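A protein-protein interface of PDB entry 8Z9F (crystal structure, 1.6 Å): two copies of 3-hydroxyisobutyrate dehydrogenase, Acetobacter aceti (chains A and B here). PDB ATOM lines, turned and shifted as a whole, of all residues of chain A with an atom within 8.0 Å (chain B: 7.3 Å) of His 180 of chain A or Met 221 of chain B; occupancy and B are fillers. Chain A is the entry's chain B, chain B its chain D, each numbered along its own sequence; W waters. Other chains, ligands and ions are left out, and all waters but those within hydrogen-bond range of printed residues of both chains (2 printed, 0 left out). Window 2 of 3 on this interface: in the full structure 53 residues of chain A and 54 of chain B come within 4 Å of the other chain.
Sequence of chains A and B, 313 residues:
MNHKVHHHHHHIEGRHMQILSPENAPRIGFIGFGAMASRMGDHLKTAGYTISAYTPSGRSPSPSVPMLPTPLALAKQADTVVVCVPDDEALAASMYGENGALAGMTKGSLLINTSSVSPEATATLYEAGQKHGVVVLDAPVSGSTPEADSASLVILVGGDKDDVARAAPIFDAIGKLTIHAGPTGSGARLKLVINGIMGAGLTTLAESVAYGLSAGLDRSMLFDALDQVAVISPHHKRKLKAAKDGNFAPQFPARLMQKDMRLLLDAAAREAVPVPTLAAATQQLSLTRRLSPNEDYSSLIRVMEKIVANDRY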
ATOM      1  N   LEU A 137      30.353  25.250   8.429  1.00  0.00           N
ATOM      2  CA  LEU A 137      28.923  25.014   8.517  1.00  0.00           C
ATOM      3  C   LEU A 137      28.488  25.389   9.921  1.00  0.00           C
ATOM      4  O   LEU A 137      29.073  24.900  10.896  1.00  0.00           O
ATOM      5  CB  LEU A 137      28.563  23.552   8.252  1.00  0.00           C
ATOM      6  CG  LEU A 137      28.900  22.919   6.907  1.00  0.00           C
ATOM      7  CD1 LEU A 137      28.410  21.490   6.907  1.00  0.00           C
ATOM      8  CD2 LEU A 137      28.228  23.718   5.803  1.00  0.00           C
ATOM      9  N   ASP A 138      27.478  26.245  10.029  1.00  0.00           N
ATOM     10  CA  ASP A 138      26.855  26.495  11.324  1.00  0.00           C
ATOM     11  C   ASP A 138      25.770  25.441  11.504  1.00  0.00           C
ATOM     12  O   ASP A 138      24.729  25.484  10.847  1.00  0.00           O
ATOM     13  CB  ASP A 138      26.319  27.926  11.458  1.00  0.00           C
ATOM     14  CG  ASP A 138      25.427  28.368  10.298  1.00  0.00           C
ATOM     15  OD1 ASP A 138      25.919  28.478   9.157  1.00  0.00           O
ATOM     16  OD2 ASP A 138      24.227  28.655  10.544  1.00  0.00           O
ATOM     17  N   VAL A 154      18.409  16.614  16.231  1.00  0.00           N
ATOM     18  CA  VAL A 154      18.035  17.234  14.969  1.00  0.00           C
ATOM     19  C   VAL A 154      19.093  18.281  14.654  1.00  0.00           C
ATOM     20  O   VAL A 154      19.311  19.207  15.447  1.00  0.00           O
ATOM     21  CB  VAL A 154      16.639  17.870  15.046  1.00  0.00           C
ATOM     22  CG1 VAL A 154      16.282  18.480  13.711  1.00  0.00           C
ATOM     23  CG2 VAL A 154      15.606  16.824  15.466  1.00  0.00           C
ATOM     24  N   ILE A 155      19.777  18.126  13.514  1.00  0.00           N
ATOM     25  CA  ILE A 155      20.832  19.050  13.117  1.00  0.00           C
ATOM     26  C   ILE A 155      20.199  20.183  12.323  1.00  0.00           C
ATOM     27  O   ILE A 155      19.428  19.936  11.393  1.00  0.00           O
ATOM     28  CB  ILE A 155      21.918  18.351  12.275  1.00  0.00           C
ATOM     29  CG1 ILE A 155      22.829  17.439  13.113  1.00  0.00           C
ATOM     30  CG2 ILE A 155      22.790  19.393  11.602  1.00  0.00           C
ATOM     31  CD1 ILE A 155      22.157  16.293  13.810  1.00  0.00           C
ATOM     32  N   LEU A 156      20.533  21.421  12.688  1.00  0.00           N
ATOM     33  CA  LEU A 156      20.021  22.635  12.045  1.00  0.00           C
ATOM     34  C   LEU A 156      21.201  23.307  11.347  1.00  0.00           C
ATOM     35  O   LEU A 156      22.009  23.979  11.990  1.00  0.00           O
ATOM     36  CB  LEU A 156      19.392  23.561  13.098  1.00  0.00           C
ATOM     37  CG  LEU A 156      18.596  22.873  14.224  1.00  0.00           C
ATOM     38  CD1 LEU A 156      18.349  23.831  15.420  1.00  0.00           C
ATOM     39  CD2 LEU A 156      17.280  22.355  13.693  1.00  0.00           C
ATOM     40  N   VAL A 157      21.326  23.143  10.031  1.00  0.00           N
ATOM     41  CA  VAL A 157      22.582  23.504   9.389  1.00  0.00           C
ATOM     42  C   VAL A 157      22.371  24.561   8.313  1.00  0.00           C
ATOM     43  O   VAL A 157      21.426  24.492   7.522  1.00  0.00           O
ATOM     44  CB  VAL A 157      23.305  22.269   8.806  1.00  0.00           C
ATOM     45  CG1 VAL A 157      22.451  21.543   7.778  1.00  0.00           C
ATOM     46  CG2 VAL A 157      24.663  22.686   8.261  1.00  0.00           C
ATOM     47  N   GLY A 158      23.261  25.543   8.307  1.00  0.00           N
ATOM     48  CA  GLY A 158      23.314  26.557   7.273  1.00  0.00           C
ATOM     49  C   GLY A 158      24.579  26.371   6.448  1.00  0.00           C
ATOM     50  O   GLY A 158      25.653  26.080   6.991  1.00  0.00           O
ATOM     51  N   GLY A 159      24.441  26.557   5.146  1.00  0.00           N
ATOM     52  CA  GLY A 159      25.591  26.449   4.273  1.00  0.00           C
ATOM     53  C   GLY A 159      25.158  26.115   2.862  1.00  0.00           C
ATOM     54  O   GLY A 159      23.969  26.060   2.549  1.00  0.00           O
ATOM     55  N   ASP A 160      26.162  25.918   2.014  1.00  0.00           N
ATOM     56  CA  ASP A 160      25.912  25.470   0.657  1.00  0.00           C
ATOM     57  C   ASP A 160      25.418  24.030   0.648  1.00  0.00           C
ATOM     58  O   ASP A 160      25.881  23.191   1.426  1.00  0.00           O
ATOM     59  CB  ASP A 160      27.183  25.597  -0.190  1.00  0.00           C
ATOM     60  CG  ASP A 160      26.902  25.486  -1.682  1.00  0.00           C
ATOM     61  OD1 ASP A 160      26.861  24.340  -2.200  1.00  0.00           O
ATOM     62  OD2 ASP A 160      26.734  26.536  -2.343  1.00  0.00           O
ATOM     63  N   LYS A 161      24.470  23.758  -0.253  1.00  0.00           N
ATOM     64  CA  LYS A 161      23.907  22.423  -0.424  1.00  0.00           C
ATOM     65  C   LYS A 161      24.983  21.344  -0.532  1.00  0.00           C
ATOM     66  O   LYS A 161      24.872  20.285   0.094  1.00  0.00           O
ATOM     67  CB  LYS A 161      23.020  22.412  -1.668  1.00  0.00           C
ATOM     68  CG  LYS A 161      22.535  21.046  -2.099  1.00  0.00           C
ATOM     69  CD  LYS A 161      21.882  21.122  -3.475  1.00  0.00           C
ATOM     70  CE  LYS A 161      20.798  20.065  -3.645  1.00  0.00           C
ATOM     71  NZ  LYS A 161      20.467  19.867  -5.092  1.00  0.00           N
ATOM     72  N   ASP A 162      26.031  21.596  -1.317  1.00  0.00           N
ATOM     73  CA  ASP A 162      27.054  20.577  -1.535  1.00  0.00           C
ATOM     74  C   ASP A 162      27.953  20.387  -0.322  1.00  0.00           C
ATOM     75  O   ASP A 162      28.442  19.275  -0.090  1.00  0.00           O
ATOM     76  CB  ASP A 162      27.904  20.927  -2.752  1.00  0.00           C
ATOM     77  CG  ASP A 162      27.115  20.868  -4.044  1.00  0.00           C
ATOM     78  OD1 ASP A 162      26.108  20.123  -4.102  1.00  0.00           O
ATOM     79  OD2 ASP A 162      27.505  21.569  -4.999  1.00  0.00           O
ATOM     80  N   ASP A 163      28.193  21.446   0.454  1.00  0.00           N
ATOM     81  CA  ASP A 163      28.964  21.281   1.682  1.00  0.00           C
ATOM     82  C   ASP A 163      28.156  20.530   2.731  1.00  0.00           C
ATOM     83  O   ASP A 163      28.698  19.685   3.456  1.00  0.00           O
ATOM     84  CB  ASP A 163      29.421  22.638   2.202  1.00  0.00           C
ATOM     85  CG  ASP A 163      30.297  23.364   1.207  1.00  0.00           C
ATOM     86  OD1 ASP A 163      31.223  22.720   0.667  1.00  0.00           O
ATOM     87  OD2 ASP A 163      30.059  24.564   0.953  1.00  0.00           O
ATOM     88  N   VAL A 164      26.850  20.792   2.807  1.00  0.00           N
ATOM     89  CA  VAL A 164      26.011  20.001   3.702  1.00  0.00           C
ATOM     90  C   VAL A 164      26.078  18.526   3.322  1.00  0.00           C
ATOM     91  O   VAL A 164      26.175  17.649   4.192  1.00  0.00           O
ATOM     92  CB  VAL A 164      24.569  20.538   3.692  1.00  0.00           C
ATOM     93  CG1 VAL A 164      23.651  19.607   4.469  1.00  0.00           C
ATOM     94  CG2 VAL A 164      24.543  21.945   4.276  1.00  0.00           C
ATOM     95  N   ALA A 165      26.079  18.233   2.016  1.00  0.00           N
ATOM     96  CA  ALA A 165      26.183  16.845   1.570  1.00  0.00           C
ATOM     97  C   ALA A 165      27.515  16.218   1.966  1.00  0.00           C
ATOM     98  O   ALA A 165      27.554  15.023   2.282  1.00  0.00           O
ATOM     99  CB  ALA A 165      25.978  16.758   0.055  1.00  0.00           C
ATOM    100  N   LEU A 177      17.840  13.399  11.997  1.00  0.00           N
ATOM    101  CA  LEU A 177      17.282  14.291  10.991  1.00  0.00           C
ATOM    102  C   LEU A 177      18.215  15.481  10.823  1.00  0.00           C
ATOM    103  O   LEU A 177      18.655  16.075  11.812  1.00  0.00           O
ATOM    104  CB  LEU A 177      15.871  14.751  11.398  1.00  0.00           C
ATOM    105  CG  LEU A 177      15.171  15.772  10.499  1.00  0.00           C
ATOM    106  CD1 LEU A 177      14.883  15.184   9.126  1.00  0.00           C
ATOM    107  CD2 LEU A 177      13.883  16.299  11.162  1.00  0.00           C
ATOM    108  N   THR A 178      18.524  15.818   9.576  1.00  0.00           N
ATOM    109  CA  THR A 178      19.306  17.001   9.245  1.00  0.00           C
ATOM    110  C   THR A 178      18.382  17.965   8.516  1.00  0.00           C
ATOM    111  O   THR A 178      17.846  17.622   7.454  1.00  0.00           O
ATOM    112  CB  THR A 178      20.512  16.627   8.377  1.00  0.00           C
ATOM    113  OG1 THR A 178      21.349  15.709   9.097  1.00  0.00           O
ATOM    114  CG2 THR A 178      21.328  17.863   8.006  1.00  0.00           C
ATOM    115  N   ILE A 179      18.157  19.145   9.098  1.00  0.00           N
ATOM    116  CA  ILE A 179      17.348  20.175   8.454  1.00  0.00           C
ATOM    117  C   ILE A 179      18.302  21.181   7.840  1.00  0.00           C
ATOM    118  O   ILE A 179      19.073  21.834   8.551  1.00  0.00           O
ATOM    119  CB  ILE A 179      16.384  20.858   9.437  1.00  0.00           C
ATOM    120  CG1 ILE A 179      15.341  19.850   9.930  1.00  0.00           C
ATOM    121  CG2 ILE A 179      15.681  22.052   8.751  1.00  0.00           C
ATOM    122  CD1 ILE A 179      14.564  20.301  11.168  1.00  0.00           C
ATOM    123  N   HIS A 180      18.262  21.303   6.518  1.00  0.00           N
ATOM    124  CA  HIS A 180      19.044  22.324   5.837  1.00  0.00           C
ATOM    125  C   HIS A 180      18.256  23.623   5.885  1.00  0.00           C
ATOM    126  O   HIS A 180      17.243  23.764   5.197  1.00  0.00           O
ATOM    127  CB  HIS A 180      19.349  21.902   4.406  1.00  0.00           C
ATOM    128  CG  HIS A 180      20.239  22.864   3.688  1.00  0.00           C
ATOM    129  ND1 HIS A 180      20.353  22.893   2.311  1.00  0.00           N
ATOM    130  CD2 HIS A 180      21.046  23.850   4.153  1.00  0.00           C
ATOM    131  CE1 HIS A 180      21.197  23.847   1.963  1.00  0.00           C
ATOM    132  NE2 HIS A 180      21.623  24.449   3.058  1.00  0.00           N
ATOM    133  N   ALA A 181      18.699  24.561   6.721  1.00  0.00           N
ATOM    134  CA  ALA A 181      17.906  25.739   7.038  1.00  0.00           C
ATOM    135  C   ALA A 181      18.093  26.873   6.045  1.00  0.00           C
ATOM    136  O   ALA A 181      17.301  27.822   6.064  1.00  0.00           O
ATOM    137  CB  ALA A 181      18.234  26.230   8.452  1.00  0.00           C
ATOM    138  N   GLY A 182      19.103  26.795   5.185  1.00  0.00           N
ATOM    139  CA  GLY A 182      19.424  27.856   4.258  1.00  0.00           C
ATOM    140  C   GLY A 182      20.923  28.033   4.148  1.00  0.00           C
ATOM    141  O   GLY A 182      21.691  27.157   4.544  1.00  0.00           O
ATOM    142  N   PRO A 183      21.364  29.181   3.626  1.00  0.00           N
ATOM    143  CA  PRO A 183      22.813  29.458   3.542  1.00  0.00           C
ATOM    144  C   PRO A 183      23.467  29.737   4.888  1.00  0.00           C
ATOM    145  O   PRO A 183      22.811  29.639   5.935  1.00  0.00           O
ATOM    146  CB  PRO A 183      22.890  30.685   2.619  1.00  0.00           C
ATOM    147  CG  PRO A 183      21.533  31.285   2.613  1.00  0.00           C
ATOM    148  CD  PRO A 183      20.537  30.209   2.967  1.00  0.00           C
ATOM    149  N   THR A 184      24.759  30.086   4.879  1.00  0.00           N
ATOM    150  CA  THR A 184      25.484  30.315   6.128  1.00  0.00           C
ATOM    151  C   THR A 184      24.717  31.260   7.042  1.00  0.00           C
ATOM    152  O   THR A 184      24.168  32.277   6.600  1.00  0.00           O
ATOM    153  CB  THR A 184      26.888  30.880   5.874  1.00  0.00           C
ATOM    154  OG1 THR A 184      27.508  31.197   7.130  1.00  0.00           O
ATOM    155  CG2 THR A 184      26.841  32.135   5.012  1.00  0.00           C
ATOM    156  N   SER A 186      21.970  30.377   8.672  1.00  0.00           N
ATOM    157  CA  SER A 186      20.579  29.949   8.825  1.00  0.00           C
ATOM    158  C   SER A 186      20.413  28.946   9.957  1.00  0.00           C
ATOM    159  O   SER A 186      19.347  28.898  10.589  1.00  0.00           O
ATOM    160  CB  SER A 186      20.052  29.349   7.516  1.00  0.00           C
ATOM    161  OG  SER A 186      20.209  30.263   6.438  1.00  0.00           O
ATOM    162  N   GLY A 187      21.430  28.114  10.195  1.00  0.00           N
ATOM    163  CA  GLY A 187      21.353  27.163  11.290  1.00  0.00           C
ATOM    164  C   GLY A 187      21.357  27.870  12.630  1.00  0.00           C
ATOM    165  O   GLY A 187      20.527  27.581  13.494  1.00  0.00           O
ATOM    166  N   ARG A 189      20.386  30.853  13.241  1.00  0.00           N
ATOM    167  CA  ARG A 189      19.112  31.548  13.423  1.00  0.00           C
ATOM    168  C   ARG A 189      17.992  30.583  13.792  1.00  0.00           C
ATOM    169  O   ARG A 189      17.161  30.894  14.657  1.00  0.00           O
ATOM    170  CB  ARG A 189      18.753  32.330  12.157  1.00  0.00           C
ATOM    171  CG  ARG A 189      19.591  33.575  11.958  1.00  0.00           C
ATOM    172  CD  ARG A 189      19.600  33.981  10.484  1.00  0.00           C
ATOM    173  NE  ARG A 189      20.237  35.274  10.266  1.00  0.00           N
ATOM    174  CZ  ARG A 189      21.541  35.502  10.370  1.00  0.00           C
ATOM    175  NH1 ARG A 189      22.396  34.531  10.668  1.00  0.00           N
ATOM    176  NH2 ARG A 189      22.002  36.735  10.169  1.00  0.00           N
ATOM    177  N   LEU A 190      17.935  29.413  13.146  1.00  0.00           N
ATOM    178  CA  LEU A 190      16.864  28.469  13.477  1.00  0.00           C
ATOM    179  C   LEU A 190      17.026  27.896  14.885  1.00  0.00           C
ATOM    180  O   LEU A 190      16.023  27.624  15.568  1.00  0.00           O
ATOM    181  CB  LEU A 190      16.810  27.352  12.431  1.00  0.00           C
ATOM    182  CG  LEU A 190      15.792  26.228  12.603  1.00  0.00           C
ATOM    183  CD1 LEU A 190      14.357  26.771  12.663  1.00  0.00           C
ATOM    184  CD2 LEU A 190      15.956  25.190  11.467  1.00  0.00           C
ATOM    185  N   VAL A 193      15.424  30.350  17.166  1.00  0.00           N
ATOM    186  CA  VAL A 193      13.963  30.196  17.148  1.00  0.00           C
ATOM    187  C   VAL A 193      13.528  29.080  18.096  1.00  0.00           C
ATOM    188  O   VAL A 193      12.624  29.262  18.922  1.00  0.00           O
ATOM    189  CB  VAL A 193      13.463  29.921  15.712  1.00  0.00           C
ATOM    190  CG1 VAL A 193      11.978  29.524  15.713  1.00  0.00           C
ATOM    191  CG2 VAL A 193      13.721  31.112  14.808  1.00  0.00           C
ATOM    192  N   GLY B 212      12.455  34.378  13.347  1.00  0.00           N
ATOM    193  CA  GLY B 212      13.073  33.599  12.279  1.00  0.00           C
ATOM    194  C   GLY B 212      12.901  34.250  10.917  1.00  0.00           C
ATOM    195  O   GLY B 212      13.851  34.343  10.130  1.00  0.00           O
ATOM    196  N   GLY B 216      15.644  36.285   8.069  1.00  0.00           N
ATOM    197  CA  GLY B 216      15.872  35.842   6.711  1.00  0.00           C
ATOM    198  C   GLY B 216      15.547  34.395   6.413  1.00  0.00           C
ATOM    199  O   GLY B 216      15.801  33.946   5.292  1.00  0.00           O
ATOM    200  N   LEU B 217      15.019  33.644   7.369  1.00  0.00           N
ATOM    201  CA  LEU B 217      14.707  32.240   7.112  1.00  0.00           C
ATOM    202  C   LEU B 217      13.530  32.101   6.159  1.00  0.00           C
ATOM    203  O   LEU B 217      12.525  32.803   6.282  1.00  0.00           O
ATOM    204  CB  LEU B 217      14.388  31.529   8.429  1.00  0.00           C
ATOM    205  CG  LEU B 217      15.565  31.479   9.398  1.00  0.00           C
ATOM    206  CD1 LEU B 217      15.138  30.695  10.632  1.00  0.00           C
ATOM    207  CD2 LEU B 217      16.805  30.840   8.768  1.00  0.00           C
ATOM    208  N   ASP B 218      13.659  31.162   5.224  1.00  0.00           N
ATOM    209  CA  ASP B 218      12.590  30.852   4.275  1.00  0.00           C
ATOM    210  C   ASP B 218      11.329  30.413   5.012  1.00  0.00           C
ATOM    211  O   ASP B 218      11.389  29.560   5.901  1.00  0.00           O
ATOM    212  CB  ASP B 218      13.073  29.737   3.343  1.00  0.00           C
ATOM    213  CG  ASP B 218      12.064  29.365   2.290  1.00  0.00           C
ATOM    214  OD1 ASP B 218      11.152  28.560   2.590  1.00  0.00           O
ATOM    215  OD2 ASP B 218      12.231  29.799   1.128  1.00  0.00           O
ATOM    216  N   ARG B 219      10.180  30.992   4.638  1.00  0.00           N
ATOM    217  CA  ARG B 219       8.954  30.742   5.391  1.00  0.00           C
ATOM    218  C   ARG B 219       8.534  29.273   5.330  1.00  0.00           C
ATOM    219  O   ARG B 219       8.147  28.682   6.348  1.00  0.00           O
ATOM    220  CB  ARG B 219       7.828  31.629   4.864  1.00  0.00           C
ATOM    221  CG  ARG B 219       6.535  31.504   5.674  1.00  0.00           C
ATOM    222  CD  ARG B 219       5.364  32.091   4.897  1.00  0.00           C
ATOM    223  NE  ARG B 219       4.159  32.202   5.724  1.00  0.00           N
ATOM    224  CZ  ARG B 219       3.126  31.370   5.682  1.00  0.00           C
ATOM    225  NH1 ARG B 219       3.094  30.338   4.846  1.00  0.00           N
ATOM    226  NH2 ARG B 219       2.091  31.584   6.499  1.00  0.00           N
ATOM    227  N   SER B 220       8.547  28.678   4.136  1.00  0.00           N
ATOM    228  CA  SER B 220       8.111  27.287   4.020  1.00  0.00           C
ATOM    229  C   SER B 220       9.046  26.358   4.788  1.00  0.00           C
ATOM    230  O   SER B 220       8.588  25.444   5.490  1.00  0.00           O
ATOM    231  CB  SER B 220       8.008  26.889   2.542  1.00  0.00           C
ATOM    232  OG  SER B 220       7.091  27.749   1.860  1.00  0.00           O
ATOM    233  N   MET B 221      10.353  26.603   4.694  1.00  0.00           N
ATOM    234  CA  MET B 221      11.329  25.808   5.436  1.00  0.00           C
ATOM    235  C   MET B 221      11.072  25.925   6.931  1.00  0.00           C
ATOM    236  O   MET B 221      11.027  24.918   7.645  1.00  0.00           O
ATOM    237  CB  MET B 221      12.745  26.283   5.085  1.00  0.00           C
ATOM    238  CG  MET B 221      13.941  25.687   5.843  1.00  0.00           C
ATOM    239  SD  MET B 221      14.138  25.915   7.624  1.00  0.00           S
ATOM    240  CE  MET B 221      14.524  27.661   7.771  1.00  0.00           C
ATOM    241  N   LEU B 222      10.888  27.155   7.409  1.00  0.00           N
ATOM    242  CA  LEU B 222      10.728  27.396   8.844  1.00  0.00           C
ATOM    243  C   LEU B 222       9.485  26.699   9.393  1.00  0.00           C
ATOM    244  O   LEU B 222       9.559  26.004  10.415  1.00  0.00           O
ATOM    245  CB  LEU B 222      10.687  28.900   9.108  1.00  0.00           C
ATOM    246  CG  LEU B 222      10.422  29.342  10.554  1.00  0.00           C
ATOM    247  CD1 LEU B 222      11.443  28.700  11.496  1.00  0.00           C
ATOM    248  CD2 LEU B 222      10.469  30.848  10.667  1.00  0.00           C
ATOM    249  N   PHE B 223       8.340  26.835   8.713  1.00  0.00           N
ATOM    250  CA  PHE B 223       7.130  26.198   9.223  1.00  0.00           C
ATOM    251  C   PHE B 223       7.279  24.682   9.233  1.00  0.00           C
ATOM    252  O   PHE B 223       6.860  24.010  10.183  1.00  0.00           O
ATOM    253  CB  PHE B 223       5.898  26.605   8.406  1.00  0.00           C
ATOM    254  CG  PHE B 223       5.263  27.904   8.841  1.00  0.00           C
ATOM    255  CD1 PHE B 223       5.924  29.121   8.649  1.00  0.00           C
ATOM    256  CD2 PHE B 223       3.985  27.919   9.412  1.00  0.00           C
ATOM    257  CE1 PHE B 223       5.344  30.328   9.036  1.00  0.00           C
ATOM    258  CE2 PHE B 223       3.392  29.141   9.799  1.00  0.00           C
ATOM    259  CZ  PHE B 223       4.076  30.342   9.610  1.00  0.00           C
ATOM    260  N   ASP B 224       7.904  24.118   8.193  1.00  0.00           N
ATOM    261  CA  ASP B 224       8.058  22.667   8.179  1.00  0.00           C
ATOM    262  C   ASP B 224       9.096  22.189   9.186  1.00  0.00           C
ATOM    263  O   ASP B 224       8.948  21.094   9.743  1.00  0.00           O
ATOM    264  CB  ASP B 224       8.450  22.177   6.794  1.00  0.00           C
ATOM    265  CG  ASP B 224       7.339  22.312   5.787  1.00  0.00           C
ATOM    266  OD1 ASP B 224       6.183  22.601   6.177  1.00  0.00           O
ATOM    267  OD2 ASP B 224       7.640  22.118   4.583  1.00  0.00           O
ATOM    268  N   ALA B 225      10.157  22.972   9.419  1.00  0.00           N
ATOM    269  CA  ALA B 225      11.170  22.571  10.389  1.00  0.00           C
ATOM    270  C   ALA B 225      10.588  22.492  11.795  1.00  0.00           C
ATOM    271  O   ALA B 225      10.895  21.565  12.559  1.00  0.00           O
ATOM    272  CB  ALA B 225      12.351  23.545  10.346  1.00  0.00           C
ATOM    273  N   LEU B 226       9.732  23.450  12.157  1.00  0.00           N
ATOM    274  CA  LEU B 226       9.188  23.452  13.504  1.00  0.00           C
ATOM    275  C   LEU B 226       8.229  22.289  13.730  1.00  0.00           C
ATOM    276  O   LEU B 226       8.061  21.847  14.870  1.00  0.00           O
ATOM    277  CB  LEU B 226       8.517  24.805  13.777  1.00  0.00           C
ATOM    278  CG  LEU B 226       9.526  25.982  13.842  1.00  0.00           C
ATOM    279  CD1 LEU B 226       8.798  27.294  14.105  1.00  0.00           C
ATOM    280  CD2 LEU B 226      10.628  25.775  14.866  1.00  0.00           C
ATOM    281  N   ASP B 227       7.636  21.734  12.669  1.00  0.00           N
ATOM    282  CA  ASP B 227       6.805  20.551  12.859  1.00  0.00           C
ATOM    283  C   ASP B 227       7.601  19.344  13.347  1.00  0.00           C
ATOM    284  O   ASP B 227       7.000  18.379  13.838  1.00  0.00           O
ATOM    285  CB  ASP B 227       6.083  20.191  11.561  1.00  0.00           C
ATOM    286  CG  ASP B 227       4.987  19.175  11.784  1.00  0.00           C
ATOM    287  OD1 ASP B 227       4.044  19.468  12.544  1.00  0.00           O
ATOM    288  OD2 ASP B 227       5.080  18.062  11.230  1.00  0.00           O
ATOM    289  N   LYS B 244       0.406  27.986   8.271  1.00  0.00           N
ATOM    290  CA  LYS B 244       1.149  27.938   7.014  1.00  0.00           C
ATOM    291  C   LYS B 244       0.200  28.166   5.841  1.00  0.00           C
ATOM    292  O   LYS B 244       0.542  28.868   4.879  1.00  0.00           O
ATOM    293  CB  LYS B 244       1.886  26.599   6.875  1.00  0.00           C
ATOM    294  CG  LYS B 244       2.900  26.577   5.706  1.00  0.00           C
ATOM    295  CD  LYS B 244       3.539  25.207   5.591  1.00  0.00           C
ATOM    296  CE  LYS B 244       4.588  25.189   4.488  1.00  0.00           C
ATOM    297  NZ  LYS B 244       4.857  23.790   4.035  1.00  0.00           N
HETATM  298  O   HOH W   1      16.304  30.059   4.667  1.00  0.00           O
HETATM  299  O   HOH W   2      18.265  32.022   5.478  1.00  0.00           O
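No position is printed for both chains.
Water W2 bridges OG of Ser 186 of chain A (2.8 Å) and O of Gly 216 of chain B (3.1 Å).
Water W1 bridges the backbone carbonyl oxygen (O) of Ala 181 of chain A (2.8 Å) and the backbone NH (N) of Asp 218 of chain B (2.9 Å).
The side-chain hydroxyl (OG) of Ser 186 of chain A lies within hydrogen-bond range of the backbone carbonyl oxygen (O) of Pro 183 of chain A, 2.7 Å away.
O of Gly 182 of chain A sits at hydrogen-bond distance from NE2 of His 180 of chain A, 3.1 Å away.
O of Val 157 of chain A is in hydrogen-bond range of N of Ala 181 of chain A.
The backbone carbonyl oxygen (O) of Ile 155 of chain A lies within hydrogen-bond range of the backbone NH (N) of Ile 179 of chain A.
The backbone NH (N) of Val 157 of chain A lies within hydrogen-bond range of the backbone carbonyl oxygen (O) of Ile 179 of chain A, at 3.0 Å.
O of Gly 212 of chain B is in hydrogen-bond range of N of Leu 217 of chain B, 3.1 Å away.
Met 221 of chain B touches just these residues of chain A: His 180 and Ala 181.
Of the printed residues of chain B, Leu 190 of chain A touches Leu 217 (3.97 Å) and Leu 222 (3.7 Å).
Of the printed residues of chain B, Val 193 of chain A touches Gly 212 (3.6 Å).
The nearest residue of chain B that does not touch His 180 of chain A is Ala 225 of chain B (7.1 Å).
The nearest printed residue of chain A that does not touch Met 221 of chain B is Ile 179 of chain A (4.3 Å).
The nearest printed residue of chain B that does not touch Leu 190 of chain A is Ala 225 of chain B (4.1 Å).
Of the 27 printed residues of chain A, 6 touch a printed residue of chain B.
Hydrophobic or aromatic side chains of chain A that line the printed part of chain B: Ile 179, Leu 190 and Val 193.
Among the printed residues, pairs that only touch across the chains: Ile 179 of chain A with Ala 225 of chain B (3.98 Å), His 180 of chain A with Met 221 of chain B (3.9 Å), Ala 181 of chain A with Met 221 of chain B (3.3 Å), Ser 186 of chain A with Leu 217 of chain B (3.7 Å), Leu 190 of chain A with Leu 217 of chain B (3.97 Å), Leu 190 of chain A with Leu 222 of chain B (3.7 Å) and Val 193 of chain A with Gly 212 of chain B (3.6 Å).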
